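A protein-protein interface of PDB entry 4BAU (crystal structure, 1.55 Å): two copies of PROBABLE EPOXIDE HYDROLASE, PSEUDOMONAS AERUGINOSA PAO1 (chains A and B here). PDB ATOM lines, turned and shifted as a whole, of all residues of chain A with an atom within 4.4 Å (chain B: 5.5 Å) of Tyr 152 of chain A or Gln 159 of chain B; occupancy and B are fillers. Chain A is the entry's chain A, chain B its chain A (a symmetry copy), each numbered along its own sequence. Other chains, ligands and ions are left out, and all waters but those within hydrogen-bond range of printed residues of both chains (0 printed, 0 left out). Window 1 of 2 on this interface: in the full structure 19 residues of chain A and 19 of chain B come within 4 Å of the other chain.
Of the printed residues of chain B, Ala 148 of chain A touches Phe 155 (3.5 Å).
Of the printed residues of chain B, Tyr 152 of chain A touches Leu 156 (3.8 Å), Gln 159 (3.5 Å) and Leu 163 (3.9 Å).
His 153 of chain A touches none of the printed residues of chain B.
Printed residues of chain B within 4 Å of Arg 182 of chain A: Gln 159.
Printed residues of chain A within 4 Å of Gln 159 of chain B: Leu 149 (2.8 Å), Tyr 152 (3.5 Å) and Arg 182 (2.7 Å).
The nearest printed residue of chain A that does not touch Gln 159 of chain B is Ala 148 of chain A (4.8 Å).
The guanidinium group (NH1) of Arg 182 of chain A is in hydrogen-bond range of the side-chain amide oxygen (OE1) of Gln 159 of chain B (2.7 Å).
O of Leu 149 of chain A is in hydrogen-bond range of NE2 of Gln 159 of chain B, at 2.8 Å.
Ala 148 of chain A touches Phe 155 of chain B.
Phe 155 of chain B touches Leu 149 of chain A.
Leu 149 of chain A touches Ala 158 of chain B.
Tyr 152 of chain A touches Leu 156 of chain B (CE2 to CD1, 3.8 Å).
Gln 159 of chain B touches Tyr 152 of chain A (NE2 to CB, 3.5 Å).
Tyr 152 of chain A touches Leu 163 of chain B.
Positions printed for both chains: 155 and 156.
Of the 8 pairs that touch across the chains among the printed residues, none has its exchanged pair printed and touching as well.
The backbone carbonyl oxygen (O) of Gln 159 of chain B is in hydrogen-bond range of the guanidinium group (NH2) of Arg 216 of chain B (2.9 Å).
O of Leu 149 of chain A sits at hydrogen-bond distance from NH2 of Arg 182 of chain A, 3.3 Å away.
The backbone carbonyl oxygen of Phe 155 of chain B is in hydrogen-bond range of the side-chain amide nitrogen of Gln 159 of chain B (2.9 Å).
The backbone carbonyl oxygen of Asn 150 of chain A is in hydrogen-bond range of the guanidinium group of Arg 182 of chain A (2.9 Å).
Of the 11 printed residues of chain A, 4 touch a printed residue of chain B.
Of the 12 printed residues of chain B, 5 touch a printed residue of chain A.
Hydrophobic or aromatic side chains of chain B that line the printed part of chain A: Phe 155, Leu 156, Ala 158 and Leu 163.
Among the printed residues, 8 pairs touch across the chains.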
ATOM      1  N   ALA A 148      10.608  25.852  15.750  1.00  0.00           N
ATOM      2  CA  ALA A 148      10.105  25.691  17.128  1.00  0.00           C
ATOM      3  C   ALA A 148      11.284  25.541  18.103  1.00  0.00           C
ATOM      4  O   ALA A 148      11.204  25.950  19.245  1.00  0.00           O
ATOM      5  CB  ALA A 148       9.112  24.512  17.247  1.00  0.00           C
ATOM      6  N   LEU A 149      12.376  24.959  17.638  1.00  0.00           N
ATOM      7  CA  LEU A 149      13.621  24.909  18.459  1.00  0.00           C
ATOM      8  C   LEU A 149      14.252  26.303  18.624  1.00  0.00           C
ATOM      9  O   LEU A 149      14.694  26.670  19.721  1.00  0.00           O
ATOM     10  CB  LEU A 149      14.599  23.891  17.879  1.00  0.00           C
ATOM     11  CG  LEU A 149      14.209  22.424  18.042  1.00  0.00           C
ATOM     12  CD1 LEU A 149      15.060  21.524  17.100  1.00  0.00           C
ATOM     13  CD2 LEU A 149      14.338  21.995  19.516  1.00  0.00           C
ATOM     14  N   ASN A 150      14.339  27.056  17.517  1.00  0.00           N
ATOM     15  CA  ASN A 150      14.944  28.399  17.524  1.00  0.00           C
ATOM     16  C   ASN A 150      14.110  29.323  18.420  1.00  0.00           C
ATOM     17  O   ASN A 150      14.620  29.940  19.349  1.00  0.00           O
ATOM     18  CB  ASN A 150      15.037  28.978  16.087  1.00  0.00           C
ATOM     19  CG  ASN A 150      16.114  28.305  15.232  1.00  0.00           C
ATOM     20  OD1 ASN A 150      16.975  27.616  15.752  1.00  0.00           O
ATOM     21  ND2 ASN A 150      16.090  28.546  13.910  1.00  0.00           N
ATOM     22  N   ALA A 151      12.805  29.343  18.160  1.00  0.00           N
ATOM     23  CA  ALA A 151      11.866  30.188  18.844  1.00  0.00           C
ATOM     24  C   ALA A 151      11.043  29.449  19.901  1.00  0.00           C
ATOM     25  O   ALA A 151       9.818  29.627  20.007  1.00  0.00           O
ATOM     26  CB  ALA A 151      10.957  30.911  17.816  1.00  0.00           C
ATOM     27  N   TYR A 152      11.714  28.653  20.723  1.00  0.00           N
ATOM     28  CA  TYR A 152      11.030  27.804  21.709  1.00  0.00           C
ATOM     29  C   TYR A 152      10.192  28.657  22.627  1.00  0.00           C
ATOM     30  O   TYR A 152       9.133  28.200  23.109  1.00  0.00           O
ATOM     31  CB  TYR A 152      12.054  26.939  22.544  1.00  0.00           C
ATOM     32  CG  TYR A 152      12.675  27.729  23.635  1.00  0.00           C
ATOM     33  CD1 TYR A 152      13.722  28.611  23.357  1.00  0.00           C
ATOM     34  CD2 TYR A 152      12.194  27.686  24.947  1.00  0.00           C
ATOM     35  CE1 TYR A 152      14.258  29.451  24.341  1.00  0.00           C
ATOM     36  CE2 TYR A 152      12.735  28.513  25.907  1.00  0.00           C
ATOM     37  CZ  TYR A 152      13.773  29.382  25.602  1.00  0.00           C
ATOM     38  OH  TYR A 152      14.201  30.202  26.626  1.00  0.00           O
ATOM     39  N   HIS A 153      10.636  29.899  22.876  1.00  0.00           N
ATOM     40  CA  HIS A 153       9.907  30.722  23.806  1.00  0.00           C
ATOM     41  C   HIS A 153       8.560  31.191  23.314  1.00  0.00           C
ATOM     42  O   HIS A 153       7.694  31.560  24.107  1.00  0.00           O
ATOM     43  CB  HIS A 153      10.752  31.916  24.277  1.00  0.00           C
ATOM     44  CG  HIS A 153      11.126  32.834  23.161  1.00  0.00           C
ATOM     45  ND1 HIS A 153      11.855  32.422  22.088  1.00  0.00           N
ATOM     46  CD2 HIS A 153      10.827  34.169  22.950  1.00  0.00           C
ATOM     47  CE1 HIS A 153      12.022  33.450  21.268  1.00  0.00           C
ATOM     48  NE2 HIS A 153      11.385  34.513  21.768  1.00  0.00           N
ATOM     49  N   TRP A 154       8.366  31.231  22.023  1.00  0.00           N
ATOM     50  CA  TRP A 154       7.062  31.542  21.461  1.00  0.00           C
ATOM     51  C   TRP A 154       6.019  30.560  21.910  1.00  0.00           C
ATOM     52  O   TRP A 154       4.838  30.893  22.012  1.00  0.00           O
ATOM     53  CB  TRP A 154       7.110  31.546  19.941  1.00  0.00           C
ATOM     54  CG  TRP A 154       7.831  32.708  19.334  1.00  0.00           C
ATOM     55  CD1 TRP A 154       8.913  33.413  19.859  1.00  0.00           C
ATOM     56  CD2 TRP A 154       7.503  33.345  18.079  1.00  0.00           C
ATOM     57  NE1 TRP A 154       9.246  34.455  19.035  1.00  0.00           N
ATOM     58  CE2 TRP A 154       8.403  34.477  17.944  1.00  0.00           C
ATOM     59  CE3 TRP A 154       6.511  33.162  17.132  1.00  0.00           C
ATOM     60  CZ2 TRP A 154       8.368  35.306  16.826  1.00  0.00           C
ATOM     61  CZ3 TRP A 154       6.493  34.004  16.011  1.00  0.00           C
ATOM     62  CH2 TRP A 154       7.365  35.045  15.877  1.00  0.00           C
ATOM     63  N   PHE A 155       6.440  29.298  22.119  1.00  0.00           N
ATOM     64  CA  PHE A 155       5.577  28.236  22.588  1.00  0.00           C
ATOM     65  C   PHE A 155       5.522  28.117  24.090  1.00  0.00           C
ATOM     66  O   PHE A 155       4.450  27.933  24.646  1.00  0.00           O
ATOM     67  CB  PHE A 155       6.039  26.953  21.861  1.00  0.00           C
ATOM     68  CG  PHE A 155       6.010  27.145  20.369  1.00  0.00           C
ATOM     69  CD1 PHE A 155       4.805  27.128  19.688  1.00  0.00           C
ATOM     70  CD2 PHE A 155       7.164  27.409  19.686  1.00  0.00           C
ATOM     71  CE1 PHE A 155       4.769  27.397  18.311  1.00  0.00           C
ATOM     72  CE2 PHE A 155       7.173  27.691  18.360  1.00  0.00           C
ATOM     73  CZ  PHE A 155       5.969  27.632  17.633  1.00  0.00           C
ATOM     74  N   LEU A 156       6.646  28.348  24.761  1.00  0.00           N
ATOM     75  CA  LEU A 156       6.640  28.349  26.230  1.00  0.00           C
ATOM     76  C   LEU A 156       5.784  29.507  26.801  1.00  0.00           C
ATOM     77  O   LEU A 156       4.933  29.269  27.665  1.00  0.00           O
ATOM     78  CB  LEU A 156       8.078  28.463  26.771  1.00  0.00           C
ATOM     79  CG  LEU A 156       8.238  28.650  28.295  1.00  0.00           C
ATOM     80  CD1 LEU A 156       7.590  27.520  29.161  1.00  0.00           C
ATOM     81  CD2 LEU A 156       9.734  28.900  28.640  1.00  0.00           C
ATOM     82  N   PHE A 175      17.409  34.656  33.257  1.00  0.00           N
ATOM     83  CA  PHE A 175      16.691  34.293  32.040  1.00  0.00           C
ATOM     84  C   PHE A 175      16.722  35.507  31.058  1.00  0.00           C
ATOM     85  O   PHE A 175      16.904  35.358  29.860  1.00  0.00           O
ATOM     86  CB  PHE A 175      15.246  33.920  32.376  1.00  0.00           C
ATOM     87  CG  PHE A 175      14.455  33.551  31.181  1.00  0.00           C
ATOM     88  CD1 PHE A 175      14.590  32.325  30.640  1.00  0.00           C
ATOM     89  CD2 PHE A 175      13.647  34.473  30.525  1.00  0.00           C
ATOM     90  CE1 PHE A 175      13.891  31.943  29.501  1.00  0.00           C
ATOM     91  CE2 PHE A 175      12.952  34.113  29.402  1.00  0.00           C
ATOM     92  CZ  PHE A 175      13.089  32.839  28.855  1.00  0.00           C
ATOM     93  N   ARG A 182      21.297  35.466  23.569  1.00  0.00           N
ATOM     94  CA  ARG A 182      20.904  34.560  22.505  1.00  0.00           C
ATOM     95  C   ARG A 182      20.360  35.375  21.305  1.00  0.00           C
ATOM     96  O   ARG A 182      20.708  35.100  20.173  1.00  0.00           O
ATOM     97  CB  ARG A 182      19.850  33.631  23.049  1.00  0.00           C
ATOM     98  CG  ARG A 182      19.270  32.693  22.054  1.00  0.00           C
ATOM     99  CD  ARG A 182      18.505  31.609  22.748  1.00  0.00           C
ATOM    100  NE  ARG A 182      17.787  30.796  21.794  1.00  0.00           N
ATOM    101  CZ  ARG A 182      17.408  29.545  22.007  1.00  0.00           C
ATOM    102  NH1 ARG A 182      17.775  28.915  23.125  1.00  0.00           N
ATOM    103  NH2 ARG A 182      16.672  28.916  21.062  1.00  0.00           N
ATOM    104  N   PHE B 155      10.440  21.174  22.811  1.00  0.00           N
ATOM    105  CA  PHE B 155      11.314  22.245  22.387  1.00  0.00           C
ATOM    106  C   PHE B 155      12.042  22.920  23.522  1.00  0.00           C
ATOM    107  O   PHE B 155      13.226  23.197  23.405  1.00  0.00           O
ATOM    108  CB  PHE B 155      10.448  23.194  21.528  1.00  0.00           C
ATOM    109  CG  PHE B 155       9.806  22.448  20.391  1.00  0.00           C
ATOM    110  CD1 PHE B 155      10.555  22.088  19.284  1.00  0.00           C
ATOM    111  CD2 PHE B 155       8.499  22.058  20.473  1.00  0.00           C
ATOM    112  CE1 PHE B 155       9.979  21.314  18.264  1.00  0.00           C
ATOM    113  CE2 PHE B 155       7.909  21.295  19.520  1.00  0.00           C
ATOM    114  CZ  PHE B 155       8.631  20.956  18.361  1.00  0.00           C
ATOM    115  N   LEU B 156      11.381  23.071  24.665  1.00  0.00           N
ATOM    116  CA  LEU B 156      12.062  23.628  25.842  1.00  0.00           C
ATOM    117  C   LEU B 156      13.193  22.696  26.346  1.00  0.00           C
ATOM    118  O   LEU B 156      14.318  23.162  26.558  1.00  0.00           O
ATOM    119  CB  LEU B 156      11.052  23.868  26.981  1.00  0.00           C
ATOM    120  CG  LEU B 156      11.630  24.290  28.348  1.00  0.00           C
ATOM    121  CD1 LEU B 156      12.491  25.596  28.316  1.00  0.00           C
ATOM    122  CD2 LEU B 156      10.492  24.337  29.408  1.00  0.00           C
ATOM    123  N   LEU B 157      12.889  21.397  26.519  1.00  0.00           N
ATOM    124  CA  LEU B 157      13.825  20.494  27.208  1.00  0.00           C
ATOM    125  C   LEU B 157      15.013  20.156  26.293  1.00  0.00           C
ATOM    126  O   LEU B 157      16.053  19.737  26.766  1.00  0.00           O
ATOM    127  CB  LEU B 157      13.111  19.237  27.678  1.00  0.00           C
ATOM    128  CG  LEU B 157      11.947  19.373  28.689  1.00  0.00           C
ATOM    129  CD1 LEU B 157      11.317  17.993  28.960  1.00  0.00           C
ATOM    130  CD2 LEU B 157      12.409  20.098  29.933  1.00  0.00           C
ATOM    131  N   ALA B 158      14.892  20.469  25.000  1.00  0.00           N
ATOM    132  CA  ALA B 158      15.953  20.246  24.012  1.00  0.00           C
ATOM    133  C   ALA B 158      16.891  21.473  23.820  1.00  0.00           C
ATOM    134  O   ALA B 158      17.832  21.392  23.051  1.00  0.00           O
ATOM    135  CB  ALA B 158      15.318  19.853  22.666  1.00  0.00           C
ATOM    136  N   GLN B 159      16.637  22.577  24.538  1.00  0.00           N
ATOM    137  CA  GLN B 159      17.452  23.748  24.424  1.00  0.00           C
ATOM    138  C   GLN B 159      18.821  23.396  25.029  1.00  0.00           C
ATOM    139  O   GLN B 159      18.929  22.475  25.844  1.00  0.00           O
ATOM    140  CB  GLN B 159      16.788  24.933  25.133  1.00  0.00           C
ATOM    141  CG  GLN B 159      15.512  25.363  24.454  1.00  0.00           C
ATOM    142  CD  GLN B 159      15.745  25.687  22.967  1.00  0.00           C
ATOM    143  OE1 GLN B 159      16.646  26.472  22.648  1.00  0.00           O
ATOM    144  NE2 GLN B 159      14.952  25.093  22.074  1.00  0.00           N
ATOM    145  N   PRO B 160      19.870  24.131  24.636  1.00  0.00           N
ATOM    146  CA  PRO B 160      21.209  23.796  25.124  1.00  0.00           C
ATOM    147  C   PRO B 160      21.362  23.832  26.652  1.00  0.00           C
ATOM    148  O   PRO B 160      20.716  24.616  27.379  1.00  0.00           O
ATOM    149  CB  PRO B 160      22.077  24.844  24.441  1.00  0.00           C
ATOM    150  CG  PRO B 160      21.293  25.256  23.223  1.00  0.00           C
ATOM    151  CD  PRO B 160      19.898  25.310  23.765  1.00  0.00           C
ATOM    152  N   TYR B 161      22.228  22.933  27.135  1.00  0.00           N
ATOM    153  CA  TYR B 161      22.557  22.872  28.534  1.00  0.00           C
ATOM    154  C   TYR B 161      23.044  24.257  28.979  1.00  0.00           C
ATOM    155  O   TYR B 161      23.862  24.879  28.262  1.00  0.00           O
ATOM    156  CB  TYR B 161      23.653  21.869  28.751  1.00  0.00           C
ATOM    157  CG  TYR B 161      24.081  21.768  30.188  1.00  0.00           C
ATOM    158  CD1 TYR B 161      23.333  21.040  31.101  1.00  0.00           C
ATOM    159  CD2 TYR B 161      25.250  22.385  30.640  1.00  0.00           C
ATOM    160  CE1 TYR B 161      23.727  20.932  32.442  1.00  0.00           C
ATOM    161  CE2 TYR B 161      25.640  22.290  31.959  1.00  0.00           C
ATOM    162  CZ  TYR B 161      24.886  21.537  32.844  1.00  0.00           C
ATOM    163  OH  TYR B 161      25.246  21.388  34.148  1.00  0.00           O
ATOM    164  N   LEU B 163      19.914  25.602  30.094  1.00  0.00           N
ATOM    165  CA  LEU B 163      18.687  26.386  30.128  1.00  0.00           C
ATOM    166  C   LEU B 163      17.462  25.688  30.721  1.00  0.00           C
ATOM    167  O   LEU B 163      16.861  26.172  31.702  1.00  0.00           O
ATOM    168  CB  LEU B 163      18.391  27.013  28.743  1.00  0.00           C
ATOM    169  CG  LEU B 163      17.125  27.871  28.504  1.00  0.00           C
ATOM    170  CD1 LEU B 163      15.783  27.186  28.498  1.00  0.00           C
ATOM    171  CD2 LEU B 163      17.120  29.081  29.449  1.00  0.00           C
ATOM    172  N   PRO B 164      17.055  24.526  30.134  1.00  0.00           N
ATOM    173  CA  PRO B 164      15.856  23.935  30.696  1.00  0.00           C
ATOM    174  C   PRO B 164      16.078  23.366  32.117  1.00  0.00           C
ATOM    175  O   PRO B 164      15.168  23.426  32.945  1.00  0.00           O
ATOM    176  CB  PRO B 164      15.503  22.828  29.705  1.00  0.00           C
ATOM    177  CG  PRO B 164      16.788  22.510  29.025  1.00  0.00           C
ATOM    178  CD  PRO B 164      17.504  23.820  28.931  1.00  0.00           C
ATOM    179  N   GLU B 165      17.288  22.943  32.429  1.00  0.00           N
ATOM    180  CA  GLU B 165      17.575  22.463  33.766  1.00  0.00           C
ATOM    181  C   GLU B 165      17.340  23.577  34.791  1.00  0.00           C
ATOM    182  O   GLU B 165      16.777  23.334  35.860  1.00  0.00           O
ATOM    183  CB  GLU B 165      19.027  21.932  33.908  1.00  0.00           C
ATOM    184  CG  GLU B 165      19.332  20.605  33.206  1.00  0.00           C
ATOM    185  CD  GLU B 165      19.732  20.686  31.746  1.00  0.00           C
ATOM    186  OE1 GLU B 165      19.522  21.731  31.051  1.00  0.00           O
ATOM    187  OE2 GLU B 165      20.246  19.633  31.263  1.00  0.00           O
ATOM    188  N   LEU B 167      15.213  26.163  34.441  1.00  0.00           N
ATOM    189  CA  LEU B 167      13.825  26.480  34.512  1.00  0.00           C
ATOM    190  C   LEU B 167      13.014  25.423  35.254  1.00  0.00           C
ATOM    191  O   LEU B 167      12.231  25.770  36.127  1.00  0.00           O
ATOM    192  CB  LEU B 167      13.262  26.781  33.141  1.00  0.00           C
ATOM    193  CG  LEU B 167      13.817  28.019  32.411  1.00  0.00           C
ATOM    194  CD1 LEU B 167      13.037  28.196  31.125  1.00  0.00           C
ATOM    195  CD2 LEU B 167      13.878  29.287  33.218  1.00  0.00           C
ATOM    196  N   ARG B 216      17.103  16.265  24.047  1.00  0.00           N
ATOM    197  CA  ARG B 216      18.156  16.734  23.141  1.00  0.00           C
ATOM    198  C   ARG B 216      18.512  15.634  22.116  1.00  0.00           C
ATOM    199  O   ARG B 216      18.707  15.907  20.937  1.00  0.00           O
ATOM    200  CB  ARG B 216      19.420  17.180  23.883  1.00  0.00           C
ATOM    201  CG  ARG B 216      19.243  18.413  24.775  1.00  0.00           C
ATOM    202  CD  ARG B 216      20.468  18.725  25.633  1.00  0.00           C
ATOM    203  NE  ARG B 216      20.189  19.913  26.404  1.00  0.00           N
ATOM    204  CZ  ARG B 216      20.125  20.011  27.735  1.00  0.00           C
ATOM    205  NH1 ARG B 216      20.610  19.054  28.522  1.00  0.00           N
ATOM    206  NH2 ARG B 216      19.665  21.136  28.268  1.00  0.00           N
